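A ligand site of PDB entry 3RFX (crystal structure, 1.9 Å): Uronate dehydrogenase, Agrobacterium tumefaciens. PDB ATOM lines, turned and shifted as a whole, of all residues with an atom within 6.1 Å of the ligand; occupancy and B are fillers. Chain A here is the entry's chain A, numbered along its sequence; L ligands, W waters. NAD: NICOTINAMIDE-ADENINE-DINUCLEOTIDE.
The backbone carbonyl oxygen (O) of Asp 34 lies within hydrogen-bond range of the backbone NH (N) of Cys 50, at 3.1 Å. The side-chain carboxylate (OD2) of Asp 34 is in hydrogen-bond range of the backbone NH (N) of Ser 36, 2.9 Å away. The side-chain carboxylate of Asp 34 is in hydrogen-bond range of the backbone NH of Ala 12 (2.9 Å). The side-chain carboxylate (OD1) of Asp 34 sits at hydrogen-bond distance from the backbone NH (N) of Ala 11. The side-chain carboxylate (OD1) of Asp 51 lies within hydrogen-bond range of the backbone NH (N) of Ala 53, 3.0 Å away. The side-chain hydroxyl (OG1) of Thr 9 sits at hydrogen-bond distance from the backbone NH (N) of Gly 72, 2.9 Å away. The backbone carbonyl oxygen of Ala 33 lies within hydrogen-bond range of the backbone NH of Gly 10 (3.1 Å).
The side-chain carboxylate (OD1) of Asp 34 sits at hydrogen-bond distance from an oxygen (O3B) of the ligand, 2.7 Å away. The backbone NH of Leu 52 sits at hydrogen-bond distance from a nitrogen (N1A) of the ligand, at 2.8 Å. An oxygen (O1A) of the ligand sits at hydrogen-bond distance from the side-chain hydroxyl (OG) of Ser 75. A nitrogen (N6A) of the ligand sits at hydrogen-bond distance from the side-chain carboxylate of Asp 51. An oxygen (O1N) of the ligand is in hydrogen-bond range of the backbone NH (N) of Leu 15, 3.0 Å away. N of Gly 73 lies within hydrogen-bond range of O4B of the ligand (3.1 Å). N of Gly 13 sits at hydrogen-bond distance from O3B of the ligand. The backbone NH of Gln 14 lies within hydrogen-bond range of an oxygen (O2A) of the ligand. The backbone NH (N) of Leu 35 lies within hydrogen-bond range of a nitrogen (N3A) of the ligand (3.3 Å). The side-chain hydroxyl (OG) of Ser 36 is in hydrogen-bond range of an oxygen (O2B) of the ligand (3.3 Å).
Water W1 bridges O3B of the ligand (2.7 Å) and OG of Ser 36 (3.4 Å). Water W4 lies within hydrogen-bond range of the backbone carbonyl oxygen of Gly 10, an oxygen (O1N) of the ligand and the backbone NH of Gly 16. Water W3 bridges a nitrogen (N6A) of the ligand (3.0 Å) and the backbone carbonyl oxygen (O) of Gln 82 (3.2 Å). Water W2 bridges N of Gly 10 (2.9 Å) and N3A of the ligand (3.0 Å).
Gly 10 touches the ligand. Ala 12 touches the ligand. O of Cys 50 touches C2A of the ligand (3.3 Å). Gly 72 touches the ligand (CA to O4B, 3.4 Å). Gly 86 touches the ligand (CA to N6A, 3.6 Å). Hydrophobic or aromatic side chains that line the ligand: Leu 15, Leu 35 and Leu 52. 15 residues have an atom within 4 Å of the ligand: Gly 10, Ala 12, Gly 13, Gln 14, Leu 15, Asp 34, Leu 35, Ser 36, Cys 50, Asp 51, Leu 52, Gly 72, Gly 73, Ser 75 and Gly 86. The nearest printed residue that does not touch the ligand is Leu 71 (4.05 Å).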
ATOM      1  N   THR A   9      -6.328 -10.316 -23.426  1.00  0.00           N
ATOM      2  CA  THR A   9      -7.004  -9.488 -22.436  1.00  0.00           C
ATOM      3  C   THR A   9      -6.648  -9.979 -21.026  1.00  0.00           C
ATOM      4  O   THR A   9      -6.101 -11.064 -20.879  1.00  0.00           O
ATOM      5  CB  THR A   9      -8.536  -9.492 -22.604  1.00  0.00           C
ATOM      6  OG1 THR A   9      -9.057 -10.795 -22.284  1.00  0.00           O
ATOM      7  CG2 THR A   9      -8.936  -9.116 -24.048  1.00  0.00           C
ATOM      8  N   GLY A  10      -6.964  -9.179 -20.012  1.00  0.00           N
ATOM      9  CA  GLY A  10      -6.583  -9.492 -18.636  1.00  0.00           C
ATOM     10  C   GLY A  10      -5.075  -9.642 -18.459  1.00  0.00           C
ATOM     11  O   GLY A  10      -4.600 -10.390 -17.590  1.00  0.00           O
ATOM     12  N   ALA A  11      -4.321  -8.909 -19.276  1.00  0.00           N
ATOM     13  CA  ALA A  11      -2.872  -9.116 -19.360  1.00  0.00           C
ATOM     14  C   ALA A  11      -2.073  -8.650 -18.127  1.00  0.00           C
ATOM     15  O   ALA A  11      -0.884  -8.923 -18.041  1.00  0.00           O
ATOM     16  CB  ALA A  11      -2.310  -8.468 -20.625  1.00  0.00           C
ATOM     17  N   ALA A  12      -2.715  -7.941 -17.220  1.00  0.00           N
ATOM     18  CA  ALA A  12      -2.036  -7.502 -16.002  1.00  0.00           C
ATOM     19  C   ALA A  12      -2.255  -8.495 -14.880  1.00  0.00           C
ATOM     20  O   ALA A  12      -1.636  -8.394 -13.818  1.00  0.00           O
ATOM     21  CB  ALA A  12      -2.525  -6.126 -15.577  1.00  0.00           C
ATOM     22  N   GLY A  13      -3.150  -9.450 -15.105  1.00  0.00           N
ATOM     23  CA  GLY A  13      -3.488 -10.444 -14.093  1.00  0.00           C
ATOM     24  C   GLY A  13      -2.431 -11.514 -14.019  1.00  0.00           C
ATOM     25  O   GLY A  13      -1.455 -11.486 -14.754  1.00  0.00           O
ATOM     26  N   GLN A  14      -2.631 -12.488 -13.137  1.00  0.00           N
ATOM     27  CA  GLN A  14      -1.618 -13.516 -12.942  1.00  0.00           C
ATOM     28  C   GLN A  14      -1.397 -14.388 -14.185  1.00  0.00           C
ATOM     29  O   GLN A  14      -0.255 -14.599 -14.591  1.00  0.00           O
ATOM     30  CB  GLN A  14      -1.943 -14.383 -11.723  1.00  0.00           C
ATOM     31  CG  GLN A  14      -0.712 -15.064 -11.129  1.00  0.00           C
ATOM     32  CD  GLN A  14      -0.979 -15.673  -9.751  1.00  0.00           C
ATOM     33  OE1 GLN A  14      -1.848 -15.208  -9.004  1.00  0.00           O
ATOM     34  NE2 GLN A  14      -0.223 -16.711  -9.420  1.00  0.00           N
ATOM     35  N   LEU A  15      -2.462 -14.884 -14.783  1.00  0.00           N
ATOM     36  CA  LEU A  15      -2.333 -15.689 -15.996  1.00  0.00           C
ATOM     37  C   LEU A  15      -1.889 -14.828 -17.192  1.00  0.00           C
ATOM     38  O   LEU A  15      -1.096 -15.267 -18.030  1.00  0.00           O
ATOM     39  CB  LEU A  15      -3.647 -16.387 -16.331  1.00  0.00           C
ATOM     40  CG  LEU A  15      -3.680 -17.911 -16.189  1.00  0.00           C
ATOM     41  CD1 LEU A  15      -3.152 -18.336 -14.822  1.00  0.00           C
ATOM     42  CD2 LEU A  15      -5.099 -18.423 -16.416  1.00  0.00           C
ATOM     43  N   GLY A  16      -2.413 -13.605 -17.252  1.00  0.00           N
ATOM     44  CA  GLY A  16      -2.055 -12.657 -18.293  1.00  0.00           C
ATOM     45  C   GLY A  16      -0.571 -12.350 -18.363  1.00  0.00           C
ATOM     46  O   GLY A  16       0.008 -12.269 -19.449  1.00  0.00           O
ATOM     47  N   ALA A  33      -4.018  -6.092 -23.156  1.00  0.00           N
ATOM     48  CA  ALA A  33      -5.024  -5.171 -22.645  1.00  0.00           C
ATOM     49  C   ALA A  33      -5.429  -5.533 -21.214  1.00  0.00           C
ATOM     50  O   ALA A  33      -5.370  -6.695 -20.817  1.00  0.00           O
ATOM     51  CB  ALA A  33      -6.253  -5.166 -23.557  1.00  0.00           C
ATOM     52  N   ASP A  34      -5.816  -4.508 -20.458  1.00  0.00           N
ATOM     53  CA  ASP A  34      -6.352  -4.713 -19.112  1.00  0.00           C
ATOM     54  C   ASP A  34      -6.984  -3.404 -18.644  1.00  0.00           C
ATOM     55  O   ASP A  34      -6.682  -2.335 -19.186  1.00  0.00           O
ATOM     56  CB  ASP A  34      -5.251  -5.150 -18.151  1.00  0.00           C
ATOM     57  CG  ASP A  34      -5.801  -5.912 -16.933  1.00  0.00           C
ATOM     58  OD1 ASP A  34      -5.510  -7.109 -16.824  1.00  0.00           O
ATOM     59  OD2 ASP A  34      -6.513  -5.310 -16.103  1.00  0.00           O
ATOM     60  N   LEU A  35      -7.872  -3.504 -17.668  1.00  0.00           N
ATOM     61  CA  LEU A  35      -8.424  -2.317 -17.017  1.00  0.00           C
ATOM     62  C   LEU A  35      -7.325  -1.657 -16.184  1.00  0.00           C
ATOM     63  O   LEU A  35      -7.273  -0.434 -16.045  1.00  0.00           O
ATOM     64  CB  LEU A  35      -9.592  -2.714 -16.117  1.00  0.00           C
ATOM     65  CG  LEU A  35     -10.275  -1.615 -15.297  1.00  0.00           C
ATOM     66  CD1 LEU A  35     -10.958  -0.606 -16.198  1.00  0.00           C
ATOM     67  CD2 LEU A  35     -11.271  -2.200 -14.317  1.00  0.00           C
ATOM     68  N   SER A  36      -6.428  -2.498 -15.645  1.00  0.00           N
ATOM     69  CA  SER A  36      -5.318  -2.041 -14.816  1.00  0.00           C
ATOM     70  C   SER A  36      -4.122  -1.603 -15.651  1.00  0.00           C
ATOM     71  O   SER A  36      -3.954  -2.057 -16.784  1.00  0.00           O
ATOM     72  CB  SER A  36      -4.878  -3.156 -13.866  1.00  0.00           C
ATOM     73  OG  SER A  36      -5.939  -3.537 -13.011  1.00  0.00           O
ATOM     74  N   CYS A  50      -8.260  -0.424 -21.067  1.00  0.00           N
ATOM     75  CA  CYS A  50      -9.682  -0.179 -21.213  1.00  0.00           C
ATOM     76  C   CYS A  50     -10.560  -1.106 -20.380  1.00  0.00           C
ATOM     77  O   CYS A  50     -10.166  -2.222 -20.033  1.00  0.00           O
ATOM     78  CB  CYS A  50     -10.109  -0.213 -22.689  1.00  0.00           C
ATOM     79  SG  CYS A  50     -10.406  -1.859 -23.382  1.00  0.00           S
ATOM     80  N   ASP A  51     -11.753  -0.615 -20.072  1.00  0.00           N
ATOM     81  CA  ASP A  51     -12.760  -1.368 -19.363  1.00  0.00           C
ATOM     82  C   ASP A  51     -13.548  -2.194 -20.376  1.00  0.00           C
ATOM     83  O   ASP A  51     -13.995  -1.665 -21.394  1.00  0.00           O
ATOM     84  CB  ASP A  51     -13.698  -0.388 -18.655  1.00  0.00           C
ATOM     85  CG  ASP A  51     -14.624  -1.056 -17.672  1.00  0.00           C
ATOM     86  OD1 ASP A  51     -14.826  -2.285 -17.764  1.00  0.00           O
ATOM     87  OD2 ASP A  51     -15.159  -0.342 -16.798  1.00  0.00           O
ATOM     88  N   LEU A  52     -13.699  -3.491 -20.120  1.00  0.00           N
ATOM     89  CA  LEU A  52     -14.497  -4.371 -20.990  1.00  0.00           C
ATOM     90  C   LEU A  52     -15.938  -3.898 -21.106  1.00  0.00           C
ATOM     91  O   LEU A  52     -16.648  -4.260 -22.055  1.00  0.00           O
ATOM     92  CB  LEU A  52     -14.443  -5.812 -20.496  1.00  0.00           C
ATOM     93  CG  LEU A  52     -13.071  -6.470 -20.670  1.00  0.00           C
ATOM     94  CD1 LEU A  52     -12.901  -7.739 -19.808  1.00  0.00           C
ATOM     95  CD2 LEU A  52     -12.817  -6.777 -22.142  1.00  0.00           C
ATOM     96  N   ALA A  53     -16.388  -3.111 -20.133  1.00  0.00           N
ATOM     97  CA  ALA A  53     -17.760  -2.640 -20.118  1.00  0.00           C
ATOM     98  C   ALA A  53     -17.958  -1.454 -21.081  1.00  0.00           C
ATOM     99  O   ALA A  53     -19.080  -1.011 -21.288  1.00  0.00           O
ATOM    100  CB  ALA A  53     -18.182  -2.249 -18.708  1.00  0.00           C
ATOM    101  N   LEU A  71      -8.623 -13.481 -21.213  1.00  0.00           N
ATOM    102  CA  LEU A  71      -8.384 -13.789 -19.797  1.00  0.00           C
ATOM    103  C   LEU A  71      -8.998 -12.726 -18.881  1.00  0.00           C
ATOM    104  O   LEU A  71      -9.129 -12.926 -17.662  1.00  0.00           O
ATOM    105  CB  LEU A  71      -6.883 -13.892 -19.533  1.00  0.00           C
ATOM    106  CG  LEU A  71      -6.140 -14.890 -20.421  1.00  0.00           C
ATOM    107  CD1 LEU A  71      -4.645 -14.861 -20.156  1.00  0.00           C
ATOM    108  CD2 LEU A  71      -6.703 -16.300 -20.249  1.00  0.00           C
ATOM    109  N   GLY A  72      -9.381 -11.599 -19.477  1.00  0.00           N
ATOM    110  CA  GLY A  72      -9.886 -10.472 -18.714  1.00  0.00           C
ATOM    111  C   GLY A  72     -11.279 -10.681 -18.138  1.00  0.00           C
ATOM    112  O   GLY A  72     -12.160 -11.232 -18.785  1.00  0.00           O
ATOM    113  N   GLY A  73     -11.470 -10.212 -16.911  1.00  0.00           N
ATOM    114  CA  GLY A  73     -12.736 -10.368 -16.238  1.00  0.00           C
ATOM    115  C   GLY A  73     -12.555 -10.744 -14.777  1.00  0.00           C
ATOM    116  O   GLY A  73     -11.445 -10.634 -14.235  1.00  0.00           O
ATOM    117  N   ILE A  74     -13.641 -11.176 -14.160  1.00  0.00           N
ATOM    118  CA  ILE A  74     -13.629 -11.542 -12.744  1.00  0.00           C
ATOM    119  C   ILE A  74     -13.528 -13.059 -12.591  1.00  0.00           C
ATOM    120  O   ILE A  74     -14.372 -13.806 -13.096  1.00  0.00           O
ATOM    121  CB  ILE A  74     -14.893 -11.056 -12.030  1.00  0.00           C
ATOM    122  CG1 ILE A  74     -15.085  -9.540 -12.235  1.00  0.00           C
ATOM    123  CG2 ILE A  74     -14.832 -11.404 -10.545  1.00  0.00           C
ATOM    124  CD1 ILE A  74     -13.994  -8.706 -11.603  1.00  0.00           C
ATOM    125  N   SER A  75     -12.500 -13.503 -11.883  1.00  0.00           N
ATOM    126  CA  SER A  75     -12.163 -14.914 -11.772  1.00  0.00           C
ATOM    127  C   SER A  75     -12.572 -15.527 -10.427  1.00  0.00           C
ATOM    128  O   SER A  75     -12.699 -16.743 -10.293  1.00  0.00           O
ATOM    129  CB  SER A  75     -10.649 -15.085 -11.957  1.00  0.00           C
ATOM    130  OG  SER A  75      -9.943 -14.193 -11.093  1.00  0.00           O
ATOM    131  N   VAL A  76     -12.745 -14.666  -9.428  1.00  0.00           N
ATOM    132  CA  VAL A  76     -13.137 -15.123  -8.099  1.00  0.00           C
ATOM    133  C   VAL A  76     -14.513 -14.565  -7.755  1.00  0.00           C
ATOM    134  O   VAL A  76     -15.025 -13.701  -8.469  1.00  0.00           O
ATOM    135  CB  VAL A  76     -12.137 -14.663  -7.035  1.00  0.00           C
ATOM    136  CG1 VAL A  76     -10.753 -15.196  -7.353  1.00  0.00           C
ATOM    137  CG2 VAL A  76     -12.122 -13.139  -6.934  1.00  0.00           C
ATOM    138  N   GLN A  82     -19.807  -5.910  -9.983  1.00  0.00           N
ATOM    139  CA  GLN A  82     -18.510  -6.051 -10.639  1.00  0.00           C
ATOM    140  C   GLN A  82     -18.510  -7.188 -11.673  1.00  0.00           C
ATOM    141  O   GLN A  82     -17.840  -7.087 -12.703  1.00  0.00           O
ATOM    142  CB  GLN A  82     -17.423  -6.328  -9.595  1.00  0.00           C
ATOM    143  CG  GLN A  82     -17.398  -5.299  -8.464  1.00  0.00           C
ATOM    144  CD  GLN A  82     -16.354  -5.625  -7.429  1.00  0.00           C
ATOM    145  OE1 GLN A  82     -15.310  -6.206  -7.733  1.00  0.00           O
ATOM    146  NE2 GLN A  82     -16.624  -5.259  -6.184  1.00  0.00           N
ATOM    147  N   GLN A  85     -20.325  -6.116 -14.894  1.00  0.00           N
ATOM    148  CA  GLN A  85     -19.498  -5.265 -15.748  1.00  0.00           C
ATOM    149  C   GLN A  85     -18.428  -6.031 -16.534  1.00  0.00           C
ATOM    150  O   GLN A  85     -18.284  -5.854 -17.741  1.00  0.00           O
ATOM    151  CB  GLN A  85     -18.851  -4.142 -14.926  1.00  0.00           C
ATOM    152  CG  GLN A  85     -19.868  -3.239 -14.239  1.00  0.00           C
ATOM    153  CD  GLN A  85     -20.557  -2.291 -15.200  1.00  0.00           C
ATOM    154  OE1 GLN A  85     -19.946  -1.771 -16.127  1.00  0.00           O
ATOM    155  NE2 GLN A  85     -21.852  -2.068 -14.981  1.00  0.00           N
ATOM    156  N   GLY A  86     -17.661  -6.875 -15.840  1.00  0.00           N
ATOM    157  CA  GLY A  86     -16.529  -7.547 -16.459  1.00  0.00           C
ATOM    158  C   GLY A  86     -16.866  -8.788 -17.265  1.00  0.00           C
ATOM    159  O   GLY A  86     -16.210  -9.087 -18.269  1.00  0.00           O
ATOM    160  N   ASN A  87     -17.897  -9.524 -16.841  1.00  0.00           N
ATOM    161  CA  ASN A  87     -18.141 -10.862 -17.375  1.00  0.00           C
ATOM    162  C   ASN A  87     -19.424 -10.998 -18.176  1.00  0.00           C
ATOM    163  O   ASN A  87     -19.625 -11.983 -18.887  1.00  0.00           O
ATOM    164  CB  ASN A  87     -18.199 -11.901 -16.236  1.00  0.00           C
ATOM    165  CG  ASN A  87     -16.870 -12.074 -15.535  1.00  0.00           C
ATOM    166  OD1 ASN A  87     -15.906 -11.351 -15.812  1.00  0.00           O
ATOM    167  ND2 ASN A  87     -16.809 -13.054 -14.641  1.00  0.00           N
ATOM    168  N   ALA A 109     -11.475 -17.885 -21.395  1.00  0.00           N
ATOM    169  CA  ALA A 109     -11.216 -18.432 -20.068  1.00  0.00           C
ATOM    170  C   ALA A 109     -12.527 -18.640 -19.318  1.00  0.00           C
ATOM    171  O   ALA A 109     -13.000 -17.757 -18.616  1.00  0.00           O
ATOM    172  CB  ALA A 109     -10.303 -17.490 -19.270  1.00  0.00           C
ATOM    173  N   ILE A 163     -11.145 -23.642 -17.062  1.00  0.00           N
ATOM    174  CA  ILE A 163      -9.857 -23.716 -16.346  1.00  0.00           C
ATOM    175  C   ILE A 163     -10.026 -24.369 -14.959  1.00  0.00           C
ATOM    176  O   ILE A 163     -10.932 -24.025 -14.211  1.00  0.00           O
ATOM    177  CB  ILE A 163      -9.237 -22.327 -16.212  1.00  0.00           C
ATOM    178  CG1 ILE A 163      -8.949 -21.746 -17.601  1.00  0.00           C
ATOM    179  CG2 ILE A 163      -7.936 -22.385 -15.407  1.00  0.00           C
ATOM    180  CD1 ILE A 163      -8.544 -20.283 -17.595  1.00  0.00           C
HETATM  181  PA  NAD L   1      -6.948 -12.317 -12.429  1.00  0.00           P
HETATM  182  O1A NAD L   1      -8.268 -11.902 -11.405  1.00  0.00           O
HETATM  183  O2A NAD L   1      -5.475 -12.720 -11.699  1.00  0.00           O
HETATM  184  O5B NAD L   1      -6.874 -11.564 -13.988  1.00  0.00           O
HETATM  185  C5B NAD L   1      -8.009 -10.870 -14.362  1.00  0.00           C
HETATM  186  C4B NAD L   1      -7.743  -9.556 -15.093  1.00  0.00           C
HETATM  187  O4B NAD L   1      -8.883  -9.046 -15.763  1.00  0.00           O
HETATM  188  C3B NAD L   1      -7.190  -8.509 -14.236  1.00  0.00           C
HETATM  189  O3B NAD L   1      -5.852  -8.177 -14.383  1.00  0.00           O
HETATM  190  C2B NAD L   1      -8.244  -7.488 -14.139  1.00  0.00           C
HETATM  191  O2B NAD L   1      -7.839  -6.150 -13.860  1.00  0.00           O
HETATM  192  C1B NAD L   1      -9.010  -7.686 -15.398  1.00  0.00           C
HETATM  193  N9A NAD L   1     -10.353  -7.193 -15.394  1.00  0.00           N
HETATM  194  C8A NAD L   1     -11.335  -7.385 -14.399  1.00  0.00           C
HETATM  195  N7A NAD L   1     -12.442  -6.652 -14.766  1.00  0.00           N
HETATM  196  C5A NAD L   1     -12.135  -5.982 -15.962  1.00  0.00           C
HETATM  197  C6A NAD L   1     -12.892  -5.099 -16.770  1.00  0.00           C
HETATM  198  N6A NAD L   1     -14.209  -4.741 -16.379  1.00  0.00           N
HETATM  199  N1A NAD L   1     -12.326  -4.581 -17.921  1.00  0.00           N
HETATM  200  C2A NAD L   1     -11.038  -4.911 -18.293  1.00  0.00           C
HETATM  201  N3A NAD L   1     -10.267  -5.814 -17.488  1.00  0.00           N
HETATM  202  C4A NAD L   1     -10.839  -6.311 -16.341  1.00  0.00           C
HETATM  203  O3  NAD L   1      -7.498 -13.674 -12.950  1.00  0.00           O
HETATM  204  PN  NAD L   1      -6.604 -14.921 -13.382  1.00  0.00           P
HETATM  205  O1N NAD L   1      -5.306 -14.475 -14.035  1.00  0.00           O
HETATM  206  O2N NAD L   1      -6.286 -15.804 -12.173  1.00  0.00           O
HETATM  207  O5D NAD L   1      -7.448 -15.762 -14.426  1.00  0.00           O
HETATM  208  O   HOH W   1      -4.682  -6.690 -12.430  1.00  0.00           O
HETATM  209  O   HOH W   2      -8.920  -7.014 -19.902  1.00  0.00           O
HETATM  210  O   HOH W   3     -15.197  -5.610 -13.682  1.00  0.00           O
HETATM  211  O   HOH W   4      -4.909 -12.669 -16.102  1.00  0.00           O
